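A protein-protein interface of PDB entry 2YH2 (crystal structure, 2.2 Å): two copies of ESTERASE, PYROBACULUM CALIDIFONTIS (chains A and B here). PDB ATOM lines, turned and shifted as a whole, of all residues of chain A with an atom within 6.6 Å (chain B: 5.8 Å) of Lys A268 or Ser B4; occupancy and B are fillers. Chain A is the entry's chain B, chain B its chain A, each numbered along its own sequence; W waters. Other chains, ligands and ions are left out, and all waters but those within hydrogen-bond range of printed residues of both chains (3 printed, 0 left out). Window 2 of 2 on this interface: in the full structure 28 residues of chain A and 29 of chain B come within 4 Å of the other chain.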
ATOM      1  N   TYR A 263     -15.272   7.013  16.029  1.00  0.00           N
ATOM      2  CA  TYR A 263     -14.534   7.907  15.142  1.00  0.00           C
ATOM      3  C   TYR A 263     -14.282   9.273  15.828  1.00  0.00           C
ATOM      4  O   TYR A 263     -13.156   9.781  15.838  1.00  0.00           O
ATOM      5  CB  TYR A 263     -15.308   8.092  13.840  1.00  0.00           C
ATOM      6  CG  TYR A 263     -14.506   8.735  12.746  1.00  0.00           C
ATOM      7  CD1 TYR A 263     -13.488   8.034  12.113  1.00  0.00           C
ATOM      8  CD2 TYR A 263     -14.758  10.029  12.339  1.00  0.00           C
ATOM      9  CE1 TYR A 263     -12.743   8.608  11.119  1.00  0.00           C
ATOM     10  CE2 TYR A 263     -14.015  10.619  11.311  1.00  0.00           C
ATOM     11  CZ  TYR A 263     -13.008   9.894  10.714  1.00  0.00           C
ATOM     12  OH  TYR A 263     -12.235  10.438   9.720  1.00  0.00           O
ATOM     13  N   ALA A 264     -15.329   9.846  16.410  1.00  0.00           N
ATOM     14  CA  ALA A 264     -15.209  11.099  17.153  1.00  0.00           C
ATOM     15  C   ALA A 264     -14.123  10.977  18.236  1.00  0.00           C
ATOM     16  O   ALA A 264     -13.252  11.842  18.368  1.00  0.00           O
ATOM     17  CB  ALA A 264     -16.557  11.469  17.785  1.00  0.00           C
ATOM     18  N   HIS A 265     -14.176   9.902  19.004  1.00  0.00           N
ATOM     19  CA  HIS A 265     -13.187   9.681  20.061  1.00  0.00           C
ATOM     20  C   HIS A 265     -11.774   9.519  19.529  1.00  0.00           C
ATOM     21  O   HIS A 265     -10.818   9.966  20.155  1.00  0.00           O
ATOM     22  CB  HIS A 265     -13.516   8.449  20.904  1.00  0.00           C
ATOM     23  CG  HIS A 265     -12.483   8.166  21.944  1.00  0.00           C
ATOM     24  ND1 HIS A 265     -12.365   8.918  23.097  1.00  0.00           N
ATOM     25  CD2 HIS A 265     -11.479   7.261  21.978  1.00  0.00           C
ATOM     26  CE1 HIS A 265     -11.339   8.478  23.801  1.00  0.00           C
ATOM     27  NE2 HIS A 265     -10.790   7.469  23.146  1.00  0.00           N
ATOM     28  N   LEU A 266     -11.624   8.844  18.401  1.00  0.00           N
ATOM     29  CA  LEU A 266     -10.294   8.630  17.854  1.00  0.00           C
ATOM     30  C   LEU A 266      -9.716   9.928  17.319  1.00  0.00           C
ATOM     31  O   LEU A 266      -8.533  10.188  17.481  1.00  0.00           O
ATOM     32  CB  LEU A 266     -10.314   7.541  16.783  1.00  0.00           C
ATOM     33  CG  LEU A 266     -10.426   6.129  17.369  1.00  0.00           C
ATOM     34  CD1 LEU A 266     -10.690   5.132  16.261  1.00  0.00           C
ATOM     35  CD2 LEU A 266      -9.157   5.755  18.141  1.00  0.00           C
ATOM     36  N   LEU A 267     -10.554  10.766  16.711  1.00  0.00           N
ATOM     37  CA  LEU A 267     -10.122  12.122  16.342  1.00  0.00           C
ATOM     38  C   LEU A 267      -9.521  12.851  17.544  1.00  0.00           C
ATOM     39  O   LEU A 267      -8.431  13.425  17.438  1.00  0.00           O
ATOM     40  CB  LEU A 267     -11.268  12.931  15.760  1.00  0.00           C
ATOM     41  CG  LEU A 267     -11.717  12.573  14.343  1.00  0.00           C
ATOM     42  CD1 LEU A 267     -13.114  13.108  14.112  1.00  0.00           C
ATOM     43  CD2 LEU A 267     -10.728  13.117  13.278  1.00  0.00           C
ATOM     44  N   LYS A 268     -10.207  12.810  18.686  1.00  0.00           N
ATOM     45  CA  LYS A 268      -9.706  13.461  19.919  1.00  0.00           C
ATOM     46  C   LYS A 268      -8.353  12.945  20.346  1.00  0.00           C
ATOM     47  O   LYS A 268      -7.525  13.713  20.838  1.00  0.00           O
ATOM     48  CB  LYS A 268     -10.646  13.249  21.109  1.00  0.00           C
ATOM     49  CG  LYS A 268     -12.028  13.833  20.991  1.00  0.00           C
ATOM     50  CD  LYS A 268     -12.845  13.431  22.207  1.00  0.00           C
ATOM     51  CE  LYS A 268     -14.192  14.133  22.255  1.00  0.00           C
ATOM     52  NZ  LYS A 268     -14.011  15.578  22.535  1.00  0.00           N
ATOM     53  N   THR A 269      -8.130  11.639  20.210  1.00  0.00           N
ATOM     54  CA  THR A 269      -6.860  11.055  20.658  1.00  0.00           C
ATOM     55  C   THR A 269      -5.705  11.543  19.768  1.00  0.00           C
ATOM     56  O   THR A 269      -4.558  11.488  20.177  1.00  0.00           O
ATOM     57  CB  THR A 269      -6.880   9.508  20.677  1.00  0.00           C
ATOM     58  OG1 THR A 269      -6.913   9.010  19.338  1.00  0.00           O
ATOM     59  CG2 THR A 269      -8.082   8.969  21.438  1.00  0.00           C
ATOM     60  N   ARG A 270      -6.000  12.005  18.553  1.00  0.00           N
ATOM     61  CA  ARG A 270      -4.979  12.623  17.696  1.00  0.00           C
ATOM     62  C   ARG A 270      -4.963  14.156  17.780  1.00  0.00           C
ATOM     63  O   ARG A 270      -4.419  14.820  16.908  1.00  0.00           O
ATOM     64  CB  ARG A 270      -5.168  12.193  16.244  1.00  0.00           C
ATOM     65  CG  ARG A 270      -5.255  10.701  16.045  1.00  0.00           C
ATOM     66  CD  ARG A 270      -4.126   9.941  16.727  1.00  0.00           C
ATOM     67  NE  ARG A 270      -2.813  10.546  16.511  1.00  0.00           N
ATOM     68  CZ  ARG A 270      -2.039  10.355  15.444  1.00  0.00           C
ATOM     69  NH1 ARG A 270      -2.434   9.586  14.435  1.00  0.00           N
ATOM     70  NH2 ARG A 270      -0.855  10.950  15.389  1.00  0.00           N
ATOM     71  N   GLY A 271      -5.556  14.716  18.830  1.00  0.00           N
ATOM     72  CA  GLY A 271      -5.538  16.159  19.049  1.00  0.00           C
ATOM     73  C   GLY A 271      -6.525  16.941  18.199  1.00  0.00           C
ATOM     74  O   GLY A 271      -6.470  18.171  18.152  1.00  0.00           O
ATOM     75  N   VAL A 272      -7.435  16.252  17.517  1.00  0.00           N
ATOM     76  CA  VAL A 272      -8.466  16.955  16.744  1.00  0.00           C
ATOM     77  C   VAL A 272      -9.670  17.182  17.656  1.00  0.00           C
ATOM     78  O   VAL A 272     -10.157  16.252  18.314  1.00  0.00           O
ATOM     79  CB  VAL A 272      -8.926  16.170  15.511  1.00  0.00           C
ATOM     80  CG1 VAL A 272      -9.991  16.963  14.752  1.00  0.00           C
ATOM     81  CG2 VAL A 272      -7.740  15.833  14.617  1.00  0.00           C
ATOM     82  N   ARG A 273     -10.136  18.422  17.695  1.00  0.00           N
ATOM     83  CA  ARG A 273     -11.349  18.762  18.407  1.00  0.00           C
ATOM     84  C   ARG A 273     -12.548  18.132  17.720  1.00  0.00           C
ATOM     85  O   ARG A 273     -12.718  18.274  16.512  1.00  0.00           O
ATOM     86  CB  ARG A 273     -11.494  20.282  18.541  1.00  0.00           C
ATOM     87  CG  ARG A 273     -10.549  20.803  19.600  1.00  0.00           C
ATOM     88  CD  ARG A 273     -10.399  22.270  19.596  1.00  0.00           C
ATOM     89  NE  ARG A 273      -9.422  22.707  20.585  1.00  0.00           N
ATOM     90  CZ  ARG A 273      -9.092  23.982  20.807  1.00  0.00           C
ATOM     91  NH1 ARG A 273      -9.667  24.974  20.109  1.00  0.00           N
ATOM     92  NH2 ARG A 273      -8.194  24.271  21.742  1.00  0.00           N
ATOM     93  N   ALA A 274     -13.354  17.412  18.503  1.00  0.00           N
ATOM     94  CA  ALA A 274     -14.452  16.623  17.968  1.00  0.00           C
ATOM     95  C   ALA A 274     -15.498  16.376  19.029  1.00  0.00           C
ATOM     96  O   ALA A 274     -15.171  16.141  20.201  1.00  0.00           O
ATOM     97  CB  ALA A 274     -13.928  15.267  17.418  1.00  0.00           C
ATOM     98  N   VAL A 275     -16.755  16.399  18.605  1.00  0.00           N
ATOM     99  CA  VAL A 275     -17.889  16.158  19.484  1.00  0.00           C
ATOM    100  C   VAL A 275     -18.786  15.111  18.838  1.00  0.00           C
ATOM    101  O   VAL A 275     -19.151  15.238  17.665  1.00  0.00           O
ATOM    102  CB  VAL A 275     -18.690  17.456  19.741  1.00  0.00           C
ATOM    103  CG1 VAL A 275     -20.007  17.167  20.515  1.00  0.00           C
ATOM    104  CG2 VAL A 275     -17.821  18.478  20.481  1.00  0.00           C
ATOM    105  N   ALA A 276     -19.109  14.067  19.597  1.00  0.00           N
ATOM    106  CA  ALA A 276     -20.158  13.144  19.234  1.00  0.00           C
ATOM    107  C   ALA A 276     -21.420  13.412  20.076  1.00  0.00           C
ATOM    108  O   ALA A 276     -21.366  13.462  21.308  1.00  0.00           O
ATOM    109  CB  ALA A 276     -19.688  11.679  19.420  1.00  0.00           C
ATOM    110  N   PRO B   2     -15.150   6.622  25.701  1.00  0.00           N
ATOM    111  CA  PRO B   2     -14.320   7.073  26.829  1.00  0.00           C
ATOM    112  C   PRO B   2     -14.456   8.570  27.141  1.00  0.00           C
ATOM    113  O   PRO B   2     -15.033   9.332  26.360  1.00  0.00           O
ATOM    114  CB  PRO B   2     -12.883   6.753  26.379  1.00  0.00           C
ATOM    115  CG  PRO B   2     -13.031   5.896  25.152  1.00  0.00           C
ATOM    116  CD  PRO B   2     -14.324   6.293  24.531  1.00  0.00           C
ATOM    117  N   LEU B   3     -13.925   8.964  28.294  1.00  0.00           N
ATOM    118  CA  LEU B   3     -13.813  10.369  28.634  1.00  0.00           C
ATOM    119  C   LEU B   3     -12.947  11.057  27.598  1.00  0.00           C
ATOM    120  O   LEU B   3     -11.931  10.512  27.174  1.00  0.00           O
ATOM    121  CB  LEU B   3     -13.180  10.569  30.021  1.00  0.00           C
ATOM    122  CG  LEU B   3     -14.141  10.633  31.205  1.00  0.00           C
ATOM    123  CD1 LEU B   3     -13.367  10.764  32.523  1.00  0.00           C
ATOM    124  CD2 LEU B   3     -15.135  11.778  31.041  1.00  0.00           C
ATOM    125  N   SER B   4     -13.357  12.257  27.193  1.00  0.00           N
ATOM    126  CA  SER B   4     -12.493  13.114  26.412  1.00  0.00           C
ATOM    127  C   SER B   4     -11.162  13.225  27.171  1.00  0.00           C
ATOM    128  O   SER B   4     -11.163  13.458  28.369  1.00  0.00           O
ATOM    129  CB  SER B   4     -13.121  14.494  26.215  1.00  0.00           C
ATOM    130  OG  SER B   4     -12.371  15.251  25.273  1.00  0.00           O
ATOM    131  N   PRO B   5     -10.034  13.029  26.478  1.00  0.00           N
ATOM    132  CA  PRO B   5      -8.714  13.110  27.093  1.00  0.00           C
ATOM    133  C   PRO B   5      -8.457  14.359  27.939  1.00  0.00           C
ATOM    134  O   PRO B   5      -7.898  14.245  29.026  1.00  0.00           O
ATOM    135  CB  PRO B   5      -7.770  13.085  25.888  1.00  0.00           C
ATOM    136  CG  PRO B   5      -8.497  12.296  24.867  1.00  0.00           C
ATOM    137  CD  PRO B   5      -9.962  12.568  25.079  1.00  0.00           C
ATOM    138  N   ILE B   6      -8.846  15.535  27.441  1.00  0.00           N
ATOM    139  CA  ILE B   6      -8.606  16.787  28.170  1.00  0.00           C
ATOM    140  C   ILE B   6      -9.389  16.792  29.467  1.00  0.00           C
ATOM    141  O   ILE B   6      -8.883  17.204  30.507  1.00  0.00           O
ATOM    142  CB  ILE B   6      -8.978  18.074  27.340  1.00  0.00           C
ATOM    143  CG1 ILE B   6      -8.537  19.353  28.069  1.00  0.00           C
ATOM    144  CG2 ILE B   6     -10.491  18.190  27.108  1.00  0.00           C
ATOM    145  CD1 ILE B   6      -7.071  19.385  28.482  1.00  0.00           C
ATOM    146  N   LEU B   7     -10.626  16.325  29.398  1.00  0.00           N
ATOM    147  CA  LEU B   7     -11.482  16.271  30.567  1.00  0.00           C
ATOM    148  C   LEU B   7     -10.892  15.304  31.572  1.00  0.00           C
ATOM    149  O   LEU B   7     -10.917  15.563  32.772  1.00  0.00           O
ATOM    150  CB  LEU B   7     -12.894  15.824  30.180  1.00  0.00           C
ATOM    151  CG  LEU B   7     -13.983  15.981  31.239  1.00  0.00           C
ATOM    152  CD1 LEU B   7     -13.918  17.353  31.876  1.00  0.00           C
ATOM    153  CD2 LEU B   7     -15.359  15.725  30.613  1.00  0.00           C
ATOM    154  N   ARG B   8     -10.356  14.199  31.061  1.00  0.00           N
ATOM    155  CA  ARG B   8      -9.687  13.200  31.873  1.00  0.00           C
ATOM    156  C   ARG B   8      -8.528  13.865  32.625  1.00  0.00           C
ATOM    157  O   ARG B   8      -8.333  13.633  33.818  1.00  0.00           O
ATOM    158  CB  ARG B   8      -9.179  12.062  30.973  1.00  0.00           C
ATOM    159  CG  ARG B   8      -8.970  10.745  31.663  1.00  0.00           C
ATOM    160  CD  ARG B   8      -8.602   9.664  30.655  1.00  0.00           C
ATOM    161  NE  ARG B   8      -8.351   8.381  31.311  1.00  0.00           N
ATOM    162  CZ  ARG B   8      -7.249   8.075  31.996  1.00  0.00           C
ATOM    163  NH1 ARG B   8      -6.252   8.954  32.131  1.00  0.00           N
ATOM    164  NH2 ARG B   8      -7.137   6.874  32.553  1.00  0.00           N
ATOM    165  N   GLN B   9      -7.791  14.714  31.909  1.00  0.00           N
ATOM    166  CA  GLN B   9      -6.676  15.478  32.460  1.00  0.00           C
ATOM    167  C   GLN B   9      -7.121  16.545  33.465  1.00  0.00           C
ATOM    168  O   GLN B   9      -6.450  16.761  34.473  1.00  0.00           O
ATOM    169  CB  GLN B   9      -5.886  16.119  31.317  1.00  0.00           C
ATOM    170  CG  GLN B   9      -4.775  17.032  31.753  1.00  0.00           C
ATOM    171  CD  GLN B   9      -3.799  17.299  30.631  1.00  0.00           C
ATOM    172  OE1 GLN B   9      -4.119  17.992  29.658  1.00  0.00           O
ATOM    173  NE2 GLN B   9      -2.597  16.747  30.754  1.00  0.00           N
ATOM    174  N   ASN B 280     -21.519  12.677  24.189  1.00  0.00           N
ATOM    175  CA  ASN B 280     -20.511  11.677  24.572  1.00  0.00           C
ATOM    176  C   ASN B 280     -19.231  12.283  25.116  1.00  0.00           C
ATOM    177  O   ASN B 280     -18.908  13.445  24.838  1.00  0.00           O
ATOM    178  CB  ASN B 280     -20.153  10.817  23.379  1.00  0.00           C
ATOM    179  CG  ASN B 280     -21.246   9.836  23.013  1.00  0.00           C
ATOM    180  OD1 ASN B 280     -22.071   9.445  23.855  1.00  0.00           O
ATOM    181  ND2 ASN B 280     -21.252   9.417  21.752  1.00  0.00           N
ATOM    182  N   GLY B 281     -18.524  11.487  25.918  1.00  0.00           N
ATOM    183  CA  GLY B 281     -17.206  11.841  26.439  1.00  0.00           C
ATOM    184  C   GLY B 281     -17.153  12.785  27.627  1.00  0.00           C
ATOM    185  O   GLY B 281     -16.064  13.102  28.119  1.00  0.00           O
ATOM    186  N   VAL B 282     -18.307  13.230  28.122  1.00  0.00           N
ATOM    187  CA  VAL B 282     -18.296  14.312  29.099  1.00  0.00           C
ATOM    188  C   VAL B 282     -19.128  14.030  30.334  1.00  0.00           C
ATOM    189  O   VAL B 282     -19.947  13.105  30.362  1.00  0.00           O
ATOM    190  CB  VAL B 282     -18.698  15.680  28.454  1.00  0.00           C
ATOM    191  CG1 VAL B 282     -17.593  16.185  27.534  1.00  0.00           C
ATOM    192  CG2 VAL B 282     -20.034  15.566  27.710  1.00  0.00           C
ATOM    193  N   LEU B 293     -13.735  22.971  26.742  1.00  0.00           N
ATOM    194  CA  LEU B 293     -14.302  21.733  26.186  1.00  0.00           C
ATOM    195  C   LEU B 293     -15.133  22.042  24.956  1.00  0.00           C
ATOM    196  O   LEU B 293     -16.097  22.828  25.040  1.00  0.00           O
ATOM    197  CB  LEU B 293     -15.227  21.032  27.177  1.00  0.00           C
ATOM    198  CG  LEU B 293     -14.643  20.358  28.414  1.00  0.00           C
ATOM    199  CD1 LEU B 293     -15.804  19.893  29.299  1.00  0.00           C
ATOM    200  CD2 LEU B 293     -13.712  19.209  28.052  1.00  0.00           C
ATOM    201  N   GLU B 294     -14.794  21.399  23.838  1.00  0.00           N
ATOM    202  CA  GLU B 294     -15.535  21.594  22.586  1.00  0.00           C
ATOM    203  C   GLU B 294     -17.004  21.200  22.718  1.00  0.00           C
ATOM    204  O   GLU B 294     -17.864  21.802  22.083  1.00  0.00           O
ATOM    205  CB  GLU B 294     -14.874  20.892  21.392  1.00  0.00           C
ATOM    206  CG  GLU B 294     -14.668  19.368  21.513  1.00  0.00           C
ATOM    207  CD  GLU B 294     -13.304  19.021  22.072  1.00  0.00           C
ATOM    208  OE1 GLU B 294     -12.858  19.741  22.985  1.00  0.00           O
ATOM    209  OE2 GLU B 294     -12.672  18.057  21.589  1.00  0.00           O
ATOM    210  N   GLU B 295     -17.296  20.236  23.589  1.00  0.00           N
ATOM    211  CA  GLU B 295     -18.673  19.820  23.835  1.00  0.00           C
ATOM    212  C   GLU B 295     -19.514  20.947  24.420  1.00  0.00           C
ATOM    213  O   GLU B 295     -20.669  21.139  24.024  1.00  0.00           O
ATOM    214  CB  GLU B 295     -18.732  18.601  24.759  1.00  0.00           C
ATOM    215  CG  GLU B 295     -18.356  17.300  24.101  1.00  0.00           C
ATOM    216  CD  GLU B 295     -16.852  17.047  24.076  1.00  0.00           C
ATOM    217  OE1 GLU B 295     -16.099  17.829  24.678  1.00  0.00           O
ATOM    218  OE2 GLU B 295     -16.428  16.064  23.442  1.00  0.00           O
HETATM  219  O   HOH W   1     -13.354  17.671  25.162  1.00  0.00           O
HETATM  220  O   HOH W   2     -17.964  14.205  22.404  1.00  0.00           O
HETATM  221  O   HOH W   3     -14.338  11.041  23.967  1.00  0.00           O
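The side-chain amino group of Lys A268 lies within salt-bridge range of the side-chain carboxylate of Glu B294, at 3.0 Å. The side-chain amino group of Lys A268 lies within salt-bridge range of the side-chain carboxylate of Glu B295, at 2.6 Å. The side-chain amino group (NZ) of Lys A268 is in hydrogen-bond range of the side-chain hydroxyl (OG) of Ser B4, 3.2 Å away. The backbone NH of Ala A274 lies within hydrogen-bond range of the side-chain carboxylate of Glu B294 (3.2 Å). The backbone NH (N) of Asn B280 lies within hydrogen-bond range of the backbone carbonyl oxygen (O) of Ala A276, 3.0 Å away. OE2 of Glu B295 lies close to O of Ala A274.
Water W1 lies within hydrogen-bond range of the side-chain hydroxyl (OG) of Ser B4 (2.6 Å), the side-chain carboxylate (OE1) of Glu B295 (2.8 Å), the side-chain carboxylate (OE1) of Glu B294 (3.0 Å) and the side-chain amino group (NZ) of Lys A268 (3.4 Å). Water W2 lies within hydrogen-bond range of the side-chain carboxylate of Glu B295 (2.6 Å), the backbone carbonyl oxygen of Asn B280 (2.7 Å) and the backbone NH of Ala A276 (3.0 Å). Water W3 lies within hydrogen-bond range of O of Pro B2 and ND1 of His A265.
Among the printed residues, pairs that only touch across the chains: His A265 with Pro B2 (3.4 Å), Val A275 with Glu B294 (3.4 Å), Arg A273 with Glu B294 (3.5 Å), Val A275 with Glu B295 (3.6 Å) and His A265 with Leu B3 (3.98 Å).
Of the 14 printed residues of chain B, 6 touch a printed residue of chain A. Of the 14 printed residues of chain A, 6 touch a printed residue of chain B.
The backbone carbonyl oxygen of Ala A274 lies within hydrogen-bond range of the side-chain amino group of Lys A268 (2.7 Å). The backbone NH (N) of Ser B4 is in hydrogen-bond range of the backbone carbonyl oxygen (O) of Gly B281, at 3.0 Å.
Thr A269 touches none of the printed residues of chain B. Printed residues of chain B within 4 Å of Ala A274: Glu B294 (3.2 Å) and Glu B295 (3.5 Å). Of the printed residues of chain B, Val A275 touches Glu B294 and Glu B295. Printed residues of chain A within 4 Å of Pro B2: His A265 (3.4 Å). Ser B4 touches just one residue of chain A: Lys A268 (3.2 Å). Gln B9 touches none of the printed residues of chain A. Printed residues of chain A within 4 Å of Glu B294: Lys A268, Arg A273, Ala A274 and Val A275. The nearest residue of chain A that does not touch Ser B4 is His A265 (5.3 Å). The nearest printed residue of chain B that does not touch His A265 is Pro B5 (4.5 Å).
No position is printed for both chains. Of the 11 pairs that touch across the chains among the printed residues, none has its exchanged pair printed and touching as well.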
